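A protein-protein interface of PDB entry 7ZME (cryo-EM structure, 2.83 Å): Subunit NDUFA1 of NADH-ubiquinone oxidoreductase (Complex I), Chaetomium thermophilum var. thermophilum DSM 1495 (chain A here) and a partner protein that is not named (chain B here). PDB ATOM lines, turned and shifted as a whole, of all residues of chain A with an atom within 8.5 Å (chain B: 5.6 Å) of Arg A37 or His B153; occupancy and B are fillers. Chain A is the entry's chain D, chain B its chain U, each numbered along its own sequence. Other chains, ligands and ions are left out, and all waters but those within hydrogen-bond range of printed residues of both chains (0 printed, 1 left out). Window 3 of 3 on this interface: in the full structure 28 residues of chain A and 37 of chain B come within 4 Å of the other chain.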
ATOM      1  N   ALA A  26     -24.672  16.913  -9.120  1.00  0.00           N
ATOM      2  CA  ALA A  26     -25.386  16.489 -10.333  1.00  0.00           C
ATOM      3  C   ALA A  26     -26.724  15.836  -9.969  1.00  0.00           C
ATOM      4  O   ALA A  26     -27.719  16.134 -10.632  1.00  0.00           O
ATOM      5  CB  ALA A  26     -24.494  15.597 -11.136  1.00  0.00           C
ATOM      6  N   ARG A  29     -29.358  18.519  -8.467  1.00  0.00           N
ATOM      7  CA  ARG A  29     -29.834  19.437  -9.536  1.00  0.00           C
ATOM      8  C   ARG A  29     -30.761  18.688 -10.487  1.00  0.00           C
ATOM      9  O   ARG A  29     -31.721  19.296 -10.933  1.00  0.00           O
ATOM     10  CB  ARG A  29     -28.661  20.132 -10.235  1.00  0.00           C
ATOM     11  CG  ARG A  29     -28.588  21.637 -10.054  1.00  0.00           C
ATOM     12  CD  ARG A  29     -27.339  22.032 -10.810  1.00  0.00           C
ATOM     13  NE  ARG A  29     -26.943  23.427 -10.744  1.00  0.00           N
ATOM     14  CZ  ARG A  29     -26.007  23.893  -9.938  1.00  0.00           C
ATOM     15  NH1 ARG A  29     -25.371  23.075  -9.117  1.00  0.00           N
ATOM     16  NH2 ARG A  29     -25.709  25.177  -9.950  1.00  0.00           N
ATOM     17  N   HIS A  30     -30.450  17.437 -10.800  1.00  0.00           N
ATOM     18  CA  HIS A  30     -31.289  16.600 -11.697  1.00  0.00           C
ATOM     19  C   HIS A  30     -32.663  16.430 -11.056  1.00  0.00           C
ATOM     20  O   HIS A  30     -33.626  16.542 -11.785  1.00  0.00           O
ATOM     21  CB  HIS A  30     -30.526  15.308 -11.990  1.00  0.00           C
ATOM     22  CG  HIS A  30     -31.082  14.408 -13.039  1.00  0.00           C
ATOM     23  ND1 HIS A  30     -31.891  13.335 -12.735  1.00  0.00           N
ATOM     24  CD2 HIS A  30     -30.879  14.360 -14.371  1.00  0.00           C
ATOM     25  CE1 HIS A  30     -32.197  12.690 -13.840  1.00  0.00           C
ATOM     26  NE2 HIS A  30     -31.596  13.304 -14.857  1.00  0.00           N
ATOM     27  N   MET A  31     -32.754  16.221  -9.741  1.00  0.00           N
ATOM     28  CA  MET A  31     -34.057  16.157  -9.029  1.00  0.00           C
ATOM     29  C   MET A  31     -34.766  17.499  -9.044  1.00  0.00           C
ATOM     30  O   MET A  31     -35.956  17.513  -9.369  1.00  0.00           O
ATOM     31  CB  MET A  31     -33.840  15.784  -7.563  1.00  0.00           C
ATOM     32  CG  MET A  31     -33.268  14.392  -7.379  1.00  0.00           C
ATOM     33  SD  MET A  31     -34.223  13.129  -8.258  1.00  0.00           S
ATOM     34  CE  MET A  31     -33.114  12.741  -9.612  1.00  0.00           C
ATOM     35  N   PHE A  32     -34.054  18.579  -8.752  1.00  0.00           N
ATOM     36  CA  PHE A  32     -34.635  19.937  -8.681  1.00  0.00           C
ATOM     37  C   PHE A  32     -35.149  20.328 -10.067  1.00  0.00           C
ATOM     38  O   PHE A  32     -36.072  21.150 -10.158  1.00  0.00           O
ATOM     39  CB  PHE A  32     -33.525  20.871  -8.211  1.00  0.00           C
ATOM     40  CG  PHE A  32     -33.945  22.212  -7.677  1.00  0.00           C
ATOM     41  CD1 PHE A  32     -34.852  22.313  -6.636  1.00  0.00           C
ATOM     42  CD2 PHE A  32     -33.394  23.375  -8.189  1.00  0.00           C
ATOM     43  CE1 PHE A  32     -35.217  23.553  -6.140  1.00  0.00           C
ATOM     44  CE2 PHE A  32     -33.758  24.613  -7.687  1.00  0.00           C
ATOM     45  CZ  PHE A  32     -34.669  24.699  -6.662  1.00  0.00           C
ATOM     46  N   ASN A  33     -34.566  19.750 -11.112  1.00  0.00           N
ATOM     47  CA  ASN A  33     -34.915  20.106 -12.505  1.00  0.00           C
ATOM     48  C   ASN A  33     -35.807  19.029 -13.112  1.00  0.00           C
ATOM     49  O   ASN A  33     -35.740  18.856 -14.323  1.00  0.00           O
ATOM     50  CB  ASN A  33     -33.663  20.400 -13.327  1.00  0.00           C
ATOM     51  CG  ASN A  33     -33.036  21.741 -13.012  1.00  0.00           C
ATOM     52  OD1 ASN A  33     -33.262  22.714 -13.723  1.00  0.00           O
ATOM     53  ND2 ASN A  33     -32.244  21.807 -11.958  1.00  0.00           N
ATOM     54  N   GLY A  34     -36.630  18.364 -12.309  1.00  0.00           N
ATOM     55  CA  GLY A  34     -37.583  17.374 -12.823  1.00  0.00           C
ATOM     56  C   GLY A  34     -36.923  16.182 -13.469  1.00  0.00           C
ATOM     57  O   GLY A  34     -37.399  15.775 -14.548  1.00  0.00           O
ATOM     58  N   ASP A  35     -35.870  15.642 -12.847  1.00  0.00           N
ATOM     59  CA  ASP A  35     -35.167  14.451 -13.378  1.00  0.00           C
ATOM     60  C   ASP A  35     -34.674  14.773 -14.782  1.00  0.00           C
ATOM     61  O   ASP A  35     -34.748  13.894 -15.650  1.00  0.00           O
ATOM     62  CB  ASP A  35     -36.056  13.213 -13.385  1.00  0.00           C
ATOM     63  CG  ASP A  35     -36.666  12.876 -12.034  1.00  0.00           C
ATOM     64  OD1 ASP A  35     -36.342  13.569 -11.049  1.00  0.00           O
ATOM     65  OD2 ASP A  35     -37.467  11.923 -11.979  1.00  0.00           O
ATOM     66  N   LYS A  36     -34.181  15.988 -14.989  1.00  0.00           N
ATOM     67  CA  LYS A  36     -33.668  16.396 -16.306  1.00  0.00           C
ATOM     68  C   LYS A  36     -32.296  16.971 -16.041  1.00  0.00           C
ATOM     69  O   LYS A  36     -32.073  17.401 -14.912  1.00  0.00           O
ATOM     70  CB  LYS A  36     -34.542  17.507 -16.886  1.00  0.00           C
ATOM     71  CG  LYS A  36     -35.914  17.091 -17.395  1.00  0.00           C
ATOM     72  CD  LYS A  36     -36.869  18.260 -17.495  1.00  0.00           C
ATOM     73  CE  LYS A  36     -38.129  17.945 -18.273  1.00  0.00           C
ATOM     74  NZ  LYS A  36     -37.887  17.946 -19.735  1.00  0.00           N
ATOM     75  N   ARG A  37     -31.416  16.975 -17.033  1.00  0.00           N
ATOM     76  CA  ARG A  37     -30.129  17.642 -16.789  1.00  0.00           C
ATOM     77  C   ARG A  37     -30.455  19.116 -16.563  1.00  0.00           C
ATOM     78  O   ARG A  37     -31.411  19.606 -17.172  1.00  0.00           O
ATOM     79  CB  ARG A  37     -29.097  17.311 -17.866  1.00  0.00           C
ATOM     80  CG  ARG A  37     -27.737  17.958 -17.658  1.00  0.00           C
ATOM     81  CD  ARG A  37     -26.562  17.138 -18.161  1.00  0.00           C
ATOM     82  NE  ARG A  37     -26.716  16.668 -19.528  1.00  0.00           N
ATOM     83  CZ  ARG A  37     -26.945  15.407 -19.873  1.00  0.00           C
ATOM     84  NH1 ARG A  37     -27.080  15.084 -21.148  1.00  0.00           N
ATOM     85  NH2 ARG A  37     -27.037  14.471 -18.946  1.00  0.00           N
ATOM     86  N   HIS A  38     -29.708  19.779 -15.692  1.00  0.00           N
ATOM     87  CA  HIS A  38     -29.949  21.204 -15.358  1.00  0.00           C
ATOM     88  C   HIS A  38     -29.496  22.081 -16.524  1.00  0.00           C
ATOM     89  O   HIS A  38     -28.947  21.543 -17.480  1.00  0.00           O
ATOM     90  CB  HIS A  38     -29.179  21.523 -14.081  1.00  0.00           C
ATOM     91  CG  HIS A  38     -27.708  21.566 -14.313  1.00  0.00           C
ATOM     92  ND1 HIS A  38     -26.964  20.428 -14.553  1.00  0.00           N
ATOM     93  CD2 HIS A  38     -26.848  22.602 -14.381  1.00  0.00           C
ATOM     94  CE1 HIS A  38     -25.711  20.760 -14.755  1.00  0.00           C
ATOM     95  NE2 HIS A  38     -25.614  22.087 -14.645  1.00  0.00           N
ATOM     96  N   ARG A  39     -29.788  23.371 -16.472  1.00  0.00           N
ATOM     97  CA  ARG A  39     -29.297  24.301 -17.513  1.00  0.00           C
ATOM     98  C   ARG A  39     -28.085  25.079 -17.002  1.00  0.00           C
ATOM     99  O   ARG A  39     -28.070  25.395 -15.827  1.00  0.00           O
ATOM    100  CB  ARG A  39     -30.422  25.270 -17.888  1.00  0.00           C
ATOM    101  CG  ARG A  39     -31.722  24.615 -18.325  1.00  0.00           C
ATOM    102  CD  ARG A  39     -31.606  23.999 -19.702  1.00  0.00           C
ATOM    103  NE  ARG A  39     -31.105  24.950 -20.678  1.00  0.00           N
ATOM    104  CZ  ARG A  39     -31.863  25.812 -21.339  1.00  0.00           C
ATOM    105  NH1 ARG A  39     -33.164  25.848 -21.114  1.00  0.00           N
ATOM    106  NH2 ARG A  39     -31.321  26.637 -22.214  1.00  0.00           N
ATOM    107  N   TRP A  40     -27.125  25.403 -17.864  1.00  0.00           N
ATOM    108  CA  TRP A  40     -25.941  26.218 -17.492  1.00  0.00           C
ATOM    109  C   TRP A  40     -25.713  27.326 -18.512  1.00  0.00           C
ATOM    110  O   TRP A  40     -26.341  27.271 -19.575  1.00  0.00           O
ATOM    111  CB  TRP A  40     -24.688  25.345 -17.351  1.00  0.00           C
ATOM    112  CG  TRP A  40     -24.264  24.552 -18.549  1.00  0.00           C
ATOM    113  CD1 TRP A  40     -23.342  24.913 -19.486  1.00  0.00           C
ATOM    114  CD2 TRP A  40     -24.694  23.227 -18.904  1.00  0.00           C
ATOM    115  NE1 TRP A  40     -23.192  23.921 -20.415  1.00  0.00           N
ATOM    116  CE2 TRP A  40     -24.009  22.874 -20.086  1.00  0.00           C
ATOM    117  CE3 TRP A  40     -25.602  22.316 -18.355  1.00  0.00           C
ATOM    118  CZ2 TRP A  40     -24.200  21.648 -20.721  1.00  0.00           C
ATOM    119  CZ3 TRP A  40     -25.793  21.107 -18.985  1.00  0.00           C
ATOM    120  CH2 TRP A  40     -25.099  20.778 -20.147  1.00  0.00           C
ATOM    121  N   ARG A  61     -38.928  24.094 -16.031  1.00  0.00           N
ATOM    122  CA  ARG A  61     -38.222  23.146 -16.921  1.00  0.00           C
ATOM    123  C   ARG A  61     -39.217  22.256 -17.657  1.00  0.00           C
ATOM    124  O   ARG A  61     -38.763  21.288 -18.273  1.00  0.00           O
ATOM    125  CB  ARG A  61     -37.252  22.320 -16.076  1.00  0.00           C
ATOM    126  CG  ARG A  61     -36.081  23.116 -15.522  1.00  0.00           C
ATOM    127  CD  ARG A  61     -35.216  23.659 -16.639  1.00  0.00           C
ATOM    128  NE  ARG A  61     -34.944  22.663 -17.665  1.00  0.00           N
ATOM    129  CZ  ARG A  61     -33.963  21.771 -17.611  1.00  0.00           C
ATOM    130  NH1 ARG A  61     -33.796  20.910 -18.597  1.00  0.00           N
ATOM    131  NH2 ARG A  61     -33.152  21.741 -16.573  1.00  0.00           N
ATOM    132  N   ASP B 103     -33.694  19.130 -24.370  1.00  0.00           N
ATOM    133  CA  ASP B 103     -33.912  19.587 -22.972  1.00  0.00           C
ATOM    134  C   ASP B 103     -32.856  19.010 -22.029  1.00  0.00           C
ATOM    135  O   ASP B 103     -32.552  19.676 -21.039  1.00  0.00           O
ATOM    136  CB  ASP B 103     -35.361  19.443 -22.499  1.00  0.00           C
ATOM    137  CG  ASP B 103     -35.736  20.568 -21.554  1.00  0.00           C
ATOM    138  OD1 ASP B 103     -35.413  21.728 -21.874  1.00  0.00           O
ATOM    139  OD2 ASP B 103     -36.310  20.276 -20.492  1.00  0.00           O
ATOM    140  N   ASN B 104     -32.385  17.791 -22.287  1.00  0.00           N
ATOM    141  CA  ASN B 104     -31.351  17.160 -21.428  1.00  0.00           C
ATOM    142  C   ASN B 104     -29.947  17.626 -21.814  1.00  0.00           C
ATOM    143  O   ASN B 104     -29.028  17.191 -21.148  1.00  0.00           O
ATOM    144  CB  ASN B 104     -31.435  15.637 -21.474  1.00  0.00           C
ATOM    145  CG  ASN B 104     -32.463  15.072 -20.520  1.00  0.00           C
ATOM    146  OD1 ASN B 104     -32.425  15.348 -19.324  1.00  0.00           O
ATOM    147  ND2 ASN B 104     -33.377  14.267 -21.038  1.00  0.00           N
ATOM    148  N   ASN B 105     -29.781  18.485 -22.823  1.00  0.00           N
ATOM    149  CA  ASN B 105     -28.448  18.850 -23.286  1.00  0.00           C
ATOM    150  C   ASN B 105     -28.257  20.360 -23.336  1.00  0.00           C
ATOM    151  O   ASN B 105     -27.558  20.867 -24.213  1.00  0.00           O
ATOM    152  CB  ASN B 105     -28.171  18.238 -24.657  1.00  0.00           C
ATOM    153  CG  ASN B 105     -28.015  16.732 -24.605  1.00  0.00           C
ATOM    154  OD1 ASN B 105     -26.906  16.216 -24.516  1.00  0.00           O
ATOM    155  ND2 ASN B 105     -29.130  16.020 -24.666  1.00  0.00           N
ATOM    156  N   GLN B 111     -25.422  18.854 -29.587  1.00  0.00           N
ATOM    157  CA  GLN B 111     -25.417  17.749 -28.604  1.00  0.00           C
ATOM    158  C   GLN B 111     -26.525  16.762 -28.951  1.00  0.00           C
ATOM    159  O   GLN B 111     -26.660  15.767 -28.230  1.00  0.00           O
ATOM    160  CB  GLN B 111     -25.632  18.324 -27.205  1.00  0.00           C
ATOM    161  CG  GLN B 111     -24.632  19.391 -26.795  1.00  0.00           C
ATOM    162  CD  GLN B 111     -23.394  18.802 -26.171  1.00  0.00           C
ATOM    163  OE1 GLN B 111     -23.117  17.615 -26.305  1.00  0.00           O
ATOM    164  NE2 GLN B 111     -22.633  19.632 -25.479  1.00  0.00           N
ATOM    165  N   PHE B 151     -17.491  19.869 -29.744  1.00  0.00           N
ATOM    166  CA  PHE B 151     -17.971  20.380 -28.436  1.00  0.00           C
ATOM    167  C   PHE B 151     -19.063  19.468 -27.885  1.00  0.00           C
ATOM    168  O   PHE B 151     -19.576  19.755 -26.789  1.00  0.00           O
ATOM    169  CB  PHE B 151     -18.299  21.870 -28.527  1.00  0.00           C
ATOM    170  CG  PHE B 151     -17.107  22.727 -28.860  1.00  0.00           C
ATOM    171  CD1 PHE B 151     -16.214  23.112 -27.873  1.00  0.00           C
ATOM    172  CD2 PHE B 151     -16.862  23.126 -30.162  1.00  0.00           C
ATOM    173  CE1 PHE B 151     -15.110  23.891 -28.177  1.00  0.00           C
ATOM    174  CE2 PHE B 151     -15.756  23.902 -30.465  1.00  0.00           C
ATOM    175  CZ  PHE B 151     -14.885  24.285 -29.474  1.00  0.00           C
ATOM    176  N   ALA B 152     -19.371  18.385 -28.601  1.00  0.00           N
ATOM    177  CA  ALA B 152     -20.398  17.419 -28.138  1.00  0.00           C
ATOM    178  C   ALA B 152     -19.810  16.528 -27.050  1.00  0.00           C
ATOM    179  O   ALA B 152     -18.757  15.932 -27.306  1.00  0.00           O
ATOM    180  CB  ALA B 152     -20.909  16.594 -29.282  1.00  0.00           C
ATOM    181  N   HIS B 153     -20.483  16.428 -25.904  1.00  0.00           N
ATOM    182  CA  HIS B 153     -19.940  15.644 -24.769  1.00  0.00           C
ATOM    183  C   HIS B 153     -19.860  14.160 -25.112  1.00  0.00           C
ATOM    184  O   HIS B 153     -18.969  13.495 -24.576  1.00  0.00           O
ATOM    185  CB  HIS B 153     -20.671  15.996 -23.474  1.00  0.00           C
ATOM    186  CG  HIS B 153     -22.157  15.966 -23.533  1.00  0.00           C
ATOM    187  ND1 HIS B 153     -22.860  14.862 -23.955  1.00  0.00           N
ATOM    188  CD2 HIS B 153     -23.075  16.884 -23.166  1.00  0.00           C
ATOM    189  CE1 HIS B 153     -24.149  15.112 -23.881  1.00  0.00           C
ATOM    190  NE2 HIS B 153     -24.305  16.347 -23.400  1.00  0.00           N
ATOM    191  N   HIS B 154     -20.743  13.680 -25.984  1.00  0.00           N
ATOM    192  CA  HIS B 154     -20.721  12.270 -26.433  1.00  0.00           C
ATOM    193  C   HIS B 154     -20.415  12.250 -27.927  1.00  0.00           C
ATOM    194  O   HIS B 154     -21.062  13.001 -28.669  1.00  0.00           O
ATOM    195  CB  HIS B 154     -22.061  11.595 -26.127  1.00  0.00           C
ATOM    196  CG  HIS B 154     -22.434  11.610 -24.684  1.00  0.00           C
ATOM    197  ND1 HIS B 154     -23.742  11.752 -24.263  1.00  0.00           N
ATOM    198  CD2 HIS B 154     -21.685  11.507 -23.564  1.00  0.00           C
ATOM    199  CE1 HIS B 154     -23.782  11.733 -22.947  1.00  0.00           C
ATOM    200  NE2 HIS B 154     -22.532  11.589 -22.494  1.00  0.00           N
ATOM    201  N   ALA B 155     -19.478  11.402 -28.347  1.00  0.00           N
ATOM    202  CA  ALA B 155     -19.074  11.339 -29.769  1.00  0.00           C
ATOM    203  C   ALA B 155     -20.218  10.787 -30.612  1.00  0.00           C
ATOM    204  O   ALA B 155     -21.002   9.991 -30.086  1.00  0.00           O
ATOM    205  CB  ALA B 155     -17.820  10.523 -29.917  1.00  0.00           C
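OD2 of Asp B103 lies within salt-bridge range of NZ of Lys A36 (2.9 Å). The side-chain carboxylate (OD2) of Asp B103 lies within salt-bridge range of the guanidinium group (NH1) of Arg A61, 3.2 Å away. NH1 of Arg A37 lies within hydrogen-bond range of O of Asn B104, at 2.9 Å.
NE2 of His B153 lies within hydrogen-bond range of OD1 of Asn B105. OE1 of Gln B111 sits at hydrogen-bond distance from N of His B153 (2.9 Å). A ring nitrogen (ND1) of His B153 sits at hydrogen-bond distance from a ring nitrogen (ND1) of His B154 (3.2 Å). N of Lys A36 lies within hydrogen-bond range of O of His A30 (3.3 Å). OD1 of Asn A33 lies within hydrogen-bond range of NH2 of Arg A61, at 3.0 Å. NH2 of Arg A61 lies within hydrogen-bond range of O of Arg A37 (2.8 Å).
Among the printed residues, pairs that only touch across the chains: Lys A36 with Asn B104 (3.4 Å), Arg A37 with Asn B105 (3.6 Å) and Arg A37 with His B153 (3.8 Å).
Of chain B, only Asn B104, Asn B105 and His B153 come within 4 Å of Arg A37. His B153 touches one residue of chain A. No residue of chain A comes within 4 Å of Ala B152. Of the printed residues of chain A, Asp B103 touches Lys A36 and Arg A61. Printed residues of chain B within 4 Å of Lys A36: Asp B103 and Asn B104. Printed residues of chain B within 4 Å of Arg A61: Asp B103. Of the printed residues of chain A, Asn B105 touches Arg A37. Of the printed residues of chain A, Asn B104 touches Lys A36 (3.4 Å) and Arg A37 (2.9 Å). Phe B151 touches none of the printed residues of chain A. The nearest residue of chain B that does not touch Arg A37 is Asp B103 (4.03 Å). The nearest residue of chain A that does not touch His B153 is Trp A40 (5.3 Å). The nearest printed residue of chain B that does not touch Arg A61 is Asn B104 (5.0 Å).
Of the 9 printed residues of chain B, 4 touch a printed residue of chain A. Hydrophobic or aromatic side chains of chain B that line the printed part of chain A: His B153. Printed residues of chain A that touch a printed residue of chain B: Lys A36, Arg A37 and Arg A61. Among the printed residues, Asp or Glu carboxylates within 4 Å of a Lys or Arg side-chain nitrogen of the other chain: Lys A36 with Asp B103 (2.9 Å) and Arg A61 with Asp B103 (3.2 Å).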
